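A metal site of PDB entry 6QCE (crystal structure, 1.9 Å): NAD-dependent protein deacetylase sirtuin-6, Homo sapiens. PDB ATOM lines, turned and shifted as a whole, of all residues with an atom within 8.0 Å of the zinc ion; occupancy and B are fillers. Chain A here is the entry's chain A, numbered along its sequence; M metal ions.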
ATOM      1  N   GLU A 134     -24.737  21.626  10.035  1.00  0.00           N
ATOM      2  CA  GLU A 134     -24.524  22.317  11.333  1.00  0.00           C
ATOM      3  C   GLU A 134     -23.083  22.099  11.842  1.00  0.00           C
ATOM      4  O   GLU A 134     -22.605  20.960  11.727  1.00  0.00           O
ATOM      5  CB  GLU A 134     -25.505  21.771  12.354  1.00  0.00           C
ATOM      6  CG  GLU A 134     -25.353  22.352  13.745  1.00  0.00           C
ATOM      7  CD  GLU A 134     -26.510  21.956  14.647  1.00  0.00           C
ATOM      8  OE1 GLU A 134     -27.673  22.351  14.355  1.00  0.00           O
ATOM      9  OE2 GLU A 134     -26.253  21.195  15.620  1.00  0.00           O
ATOM     10  N   CYS A 135     -22.441  23.140  12.423  1.00  0.00           N
ATOM     11  CA  CYS A 135     -21.072  23.004  13.003  1.00  0.00           C
ATOM     12  C   CYS A 135     -21.206  22.261  14.352  1.00  0.00           C
ATOM     13  O   CYS A 135     -21.924  22.803  15.250  1.00  0.00           O
ATOM     14  CB  CYS A 135     -20.354  24.334  13.179  1.00  0.00           C
ATOM     15  SG  CYS A 135     -18.713  24.266  13.980  1.00  0.00           S
ATOM     16  N   ALA A 136     -20.563  21.091  14.449  1.00  0.00           N
ATOM     17  CA  ALA A 136     -20.363  20.297  15.690  1.00  0.00           C
ATOM     18  C   ALA A 136     -19.767  21.193  16.798  1.00  0.00           C
ATOM     19  O   ALA A 136     -20.213  21.069  17.944  1.00  0.00           O
ATOM     20  CB  ALA A 136     -19.475  19.110  15.403  1.00  0.00           C
ATOM     21  N   LYS A 137     -18.819  22.079  16.479  1.00  0.00           N
ATOM     22  CA  LYS A 137     -18.177  22.970  17.490  1.00  0.00           C
ATOM     23  C   LYS A 137     -19.145  24.086  17.875  1.00  0.00           C
ATOM     24  O   LYS A 137     -19.736  23.964  18.959  1.00  0.00           O
ATOM     25  CB  LYS A 137     -16.827  23.514  17.008  1.00  0.00           C
ATOM     26  CG  LYS A 137     -15.662  22.537  17.125  1.00  0.00           C
ATOM     27  CD  LYS A 137     -14.301  23.135  16.857  1.00  0.00           C
ATOM     28  CE  LYS A 137     -13.223  22.081  16.647  1.00  0.00           C
ATOM     29  NZ  LYS A 137     -11.950  22.671  16.176  1.00  0.00           N
ATOM     30  N   CYS A 138     -19.328  25.098  17.020  1.00  0.00           N
ATOM     31  CA  CYS A 138     -20.075  26.337  17.380  1.00  0.00           C
ATOM     32  C   CYS A 138     -21.592  26.219  17.130  1.00  0.00           C
ATOM     33  O   CYS A 138     -22.276  27.161  17.487  1.00  0.00           O
ATOM     34  CB  CYS A 138     -19.518  27.541  16.626  1.00  0.00           C
ATOM     35  SG  CYS A 138     -19.751  27.464  14.830  1.00  0.00           S
ATOM     36  N   LYS A 139     -22.092  25.134  16.530  1.00  0.00           N
ATOM     37  CA  LYS A 139     -23.542  24.868  16.284  1.00  0.00           C
ATOM     38  C   LYS A 139     -24.102  25.747  15.147  1.00  0.00           C
ATOM     39  O   LYS A 139     -25.341  25.716  14.949  1.00  0.00           O
ATOM     40  CB  LYS A 139     -24.336  25.092  17.577  1.00  0.00           C
ATOM     41  CG  LYS A 139     -24.108  23.984  18.587  1.00  0.00           C
ATOM     42  CD  LYS A 139     -25.227  22.973  18.647  1.00  0.00           C
ATOM     43  CE  LYS A 139     -24.774  21.529  18.650  1.00  0.00           C
ATOM     44  NZ  LYS A 139     -23.607  21.294  19.532  1.00  0.00           N
ATOM     45  N   THR A 140     -23.265  26.524  14.456  1.00  0.00           N
ATOM     46  CA  THR A 140     -23.725  27.416  13.362  1.00  0.00           C
ATOM     47  C   THR A 140     -24.284  26.517  12.254  1.00  0.00           C
ATOM     48  O   THR A 140     -23.584  25.600  11.839  1.00  0.00           O
ATOM     49  CB  THR A 140     -22.635  28.360  12.823  1.00  0.00           C
ATOM     50  OG1 THR A 140     -22.291  29.325  13.816  1.00  0.00           O
ATOM     51  CG2 THR A 140     -23.082  29.135  11.592  1.00  0.00           C
ATOM     52  N   GLN A 141     -25.466  26.856  11.771  1.00  0.00           N
ATOM     53  CA  GLN A 141     -26.165  26.181  10.646  1.00  0.00           C
ATOM     54  C   GLN A 141     -25.915  26.910   9.336  1.00  0.00           C
ATOM     55  O   GLN A 141     -25.851  28.154   9.321  1.00  0.00           O
ATOM     56  CB  GLN A 141     -27.641  26.086  10.999  1.00  0.00           C
ATOM     57  CG  GLN A 141     -27.861  25.086  12.108  1.00  0.00           C
ATOM     58  CD  GLN A 141     -29.303  24.734  12.321  1.00  0.00           C
ATOM     59  OE1 GLN A 141     -30.170  25.589  12.171  1.00  0.00           O
ATOM     60  NE2 GLN A 141     -29.533  23.482  12.698  1.00  0.00           N
ATOM     61  N   TYR A 142     -25.767  26.150   8.267  1.00  0.00           N
ATOM     62  CA  TYR A 142     -25.593  26.656   6.891  1.00  0.00           C
ATOM     63  C   TYR A 142     -26.739  26.114   6.031  1.00  0.00           C
ATOM     64  O   TYR A 142     -26.911  24.913   6.004  1.00  0.00           O
ATOM     65  CB  TYR A 142     -24.236  26.238   6.345  1.00  0.00           C
ATOM     66  CG  TYR A 142     -23.041  26.716   7.140  1.00  0.00           C
ATOM     67  CD1 TYR A 142     -22.701  26.141   8.356  1.00  0.00           C
ATOM     68  CD2 TYR A 142     -22.268  27.781   6.670  1.00  0.00           C
ATOM     69  CE1 TYR A 142     -21.623  26.590   9.092  1.00  0.00           C
ATOM     70  CE2 TYR A 142     -21.181  28.245   7.393  1.00  0.00           C
ATOM     71  CZ  TYR A 142     -20.866  27.652   8.617  1.00  0.00           C
ATOM     72  OH  TYR A 142     -19.791  28.116   9.301  1.00  0.00           O
ATOM     73  N   LEU A 159     -15.811  22.297   6.445  1.00  0.00           N
ATOM     74  CA  LEU A 159     -15.454  22.922   7.744  1.00  0.00           C
ATOM     75  C   LEU A 159     -16.214  24.228   7.918  1.00  0.00           C
ATOM     76  O   LEU A 159     -16.533  24.895   6.892  1.00  0.00           O
ATOM     77  CB  LEU A 159     -13.938  23.172   7.804  1.00  0.00           C
ATOM     78  CG  LEU A 159     -13.033  21.956   7.710  1.00  0.00           C
ATOM     79  CD1 LEU A 159     -11.608  22.308   8.138  1.00  0.00           C
ATOM     80  CD2 LEU A 159     -13.566  20.789   8.539  1.00  0.00           C
ATOM     81  N   CYS A 160     -16.447  24.601   9.167  1.00  0.00           N
ATOM     82  CA  CYS A 160     -17.064  25.865   9.602  1.00  0.00           C
ATOM     83  C   CYS A 160     -16.168  27.059   9.208  1.00  0.00           C
ATOM     84  O   CYS A 160     -14.938  26.954   9.338  1.00  0.00           O
ATOM     85  CB  CYS A 160     -17.316  25.810  11.106  1.00  0.00           C
ATOM     86  SG  CYS A 160     -18.302  27.206  11.667  1.00  0.00           S
ATOM     87  N   THR A 161     -16.781  28.140   8.717  1.00  0.00           N
ATOM     88  CA  THR A 161     -16.144  29.372   8.221  1.00  0.00           C
ATOM     89  C   THR A 161     -16.453  30.547   9.172  1.00  0.00           C
ATOM     90  O   THR A 161     -16.038  31.638   8.838  1.00  0.00           O
ATOM     91  CB  THR A 161     -16.594  29.686   6.783  1.00  0.00           C
ATOM     92  OG1 THR A 161     -18.004  29.957   6.754  1.00  0.00           O
ATOM     93  CG2 THR A 161     -16.279  28.568   5.829  1.00  0.00           C
ATOM     94  N   VAL A 162     -17.112  30.335  10.309  1.00  0.00           N
ATOM     95  CA  VAL A 162     -17.382  31.430  11.303  1.00  0.00           C
ATOM     96  C   VAL A 162     -16.058  32.103  11.722  1.00  0.00           C
ATOM     97  O   VAL A 162     -15.047  31.370  11.816  1.00  0.00           O
ATOM     98  CB  VAL A 162     -18.166  30.928  12.535  1.00  0.00           C
ATOM     99  CG1 VAL A 162     -18.242  31.961  13.650  1.00  0.00           C
ATOM    100  CG2 VAL A 162     -19.568  30.493  12.144  1.00  0.00           C
ATOM    101  N   ALA A 163     -16.118  33.418  12.002  1.00  0.00           N
ATOM    102  CA  ALA A 163     -14.996  34.352  12.267  1.00  0.00           C
ATOM    103  C   ALA A 163     -14.691  34.410  13.771  1.00  0.00           C
ATOM    104  O   ALA A 163     -14.056  33.453  14.272  1.00  0.00           O
ATOM    105  CB  ALA A 163     -15.372  35.731  11.742  1.00  0.00           C
ATOM    106  N   CYS A 171     -13.196  29.266  13.101  1.00  0.00           N
ATOM    107  CA  CYS A 171     -13.665  28.130  13.932  1.00  0.00           C
ATOM    108  C   CYS A 171     -13.166  26.788  13.387  1.00  0.00           C
ATOM    109  O   CYS A 171     -12.641  25.989  14.168  1.00  0.00           O
ATOM    110  CB  CYS A 171     -15.190  28.126  14.036  1.00  0.00           C
ATOM    111  SG  CYS A 171     -15.861  26.539  14.571  1.00  0.00           S
ATOM    112  N   ARG A 172     -13.367  26.527  12.086  1.00  0.00           N
ATOM    113  CA  ARG A 172     -12.945  25.307  11.343  1.00  0.00           C
ATOM    114  C   ARG A 172     -13.568  24.019  11.909  1.00  0.00           C
ATOM    115  O   ARG A 172     -13.105  22.912  11.506  1.00  0.00           O
ATOM    116  CB  ARG A 172     -11.419  25.182  11.282  1.00  0.00           C
ATOM    117  CG  ARG A 172     -10.750  26.281  10.477  1.00  0.00           C
ATOM    118  CD  ARG A 172      -9.245  26.087  10.487  1.00  0.00           C
ATOM    119  NE  ARG A 172      -8.685  25.996   9.146  1.00  0.00           N
ATOM    120  CZ  ARG A 172      -7.531  25.389   8.830  1.00  0.00           C
ATOM    121  NH1 ARG A 172      -6.812  24.786   9.758  1.00  0.00           N
ATOM    122  NH2 ARG A 172      -7.113  25.384   7.581  1.00  0.00           N
ATOM    123  N   GLY A 173     -14.635  24.122  12.700  1.00  0.00           N
ATOM    124  CA  GLY A 173     -15.430  22.955  13.148  1.00  0.00           C
ATOM    125  C   GLY A 173     -15.862  22.089  11.980  1.00  0.00           C
ATOM    126  O   GLY A 173     -16.004  22.640  10.842  1.00  0.00           O
ATOM    127  N   GLU A 174     -16.067  20.792  12.247  1.00  0.00           N
ATOM    128  CA  GLU A 174     -16.609  19.771  11.313  1.00  0.00           C
ATOM    129  C   GLU A 174     -18.104  20.098  11.099  1.00  0.00           C
ATOM    130  O   GLU A 174     -18.814  20.360  12.116  1.00  0.00           O
ATOM    131  CB  GLU A 174     -16.393  18.391  11.927  1.00  0.00           C
ATOM    132  CG  GLU A 174     -16.560  17.221  10.980  1.00  0.00           C
ATOM    133  CD  GLU A 174     -16.225  15.898  11.672  1.00  0.00           C
ATOM    134  OE1 GLU A 174     -15.620  15.954  12.754  1.00  0.00           O
ATOM    135  OE2 GLU A 174     -16.576  14.832  11.131  1.00  0.00           O
ATOM    136  N   LEU A 175     -18.539  20.140   9.830  1.00  0.00           N
ATOM    137  CA  LEU A 175     -19.970  20.306   9.506  1.00  0.00           C
ATOM    138  C   LEU A 175     -20.569  18.914   9.328  1.00  0.00           C
ATOM    139  O   LEU A 175     -19.893  18.047   8.731  1.00  0.00           O
ATOM    140  CB  LEU A 175     -20.130  21.142   8.242  1.00  0.00           C
ATOM    141  CG  LEU A 175     -19.470  22.525   8.247  1.00  0.00           C
ATOM    142  CD1 LEU A 175     -19.882  23.298   7.006  1.00  0.00           C
ATOM    143  CD2 LEU A 175     -19.783  23.309   9.499  1.00  0.00           C
HETATM  144 ZN    ZN M   1     -18.272  26.492  13.853  1.00  0.00          ZN
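The zinc ion is bound by the side-chain sulfur of Cys 138 (2.0 Å), the side-chain sulfur of Cys 135 (2.3 Å), the side-chain sulfur of Cys 160 (2.3 Å) and the side-chain sulfur of Cys 171 (2.5 Å).
Within 4 Å of the zinc ion: Cys 135, Cys 138, Cys 160 and Cys 171.
N of Val 162 sits close to SG of Cys 160 (3.6 Å).
N of Cys 160 lies within hydrogen-bond range of O of Gly 173 (2.6 Å).
N of Cys 171 lies within hydrogen-bond range of O of Val 162 (3.1 Å).
N of Cys 135 is in hydrogen-bond range of O of Thr 140 (2.8 Å).
The backbone NH of Arg 172 is in hydrogen-bond range of the backbone carbonyl oxygen of Cys 160 (3.2 Å).
The side-chain sulfur (SG) of Cys 138 sits close to the side-chain hydroxyl (OG1) of Thr 140, at 3.3 Å.
N of Lys 137 lies close to SG of Cys 135, 3.3 Å away.
The side-chain sulfur (SG) of Cys 171 lies close to the backbone NH (N) of Gly 173 (3.3 Å).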
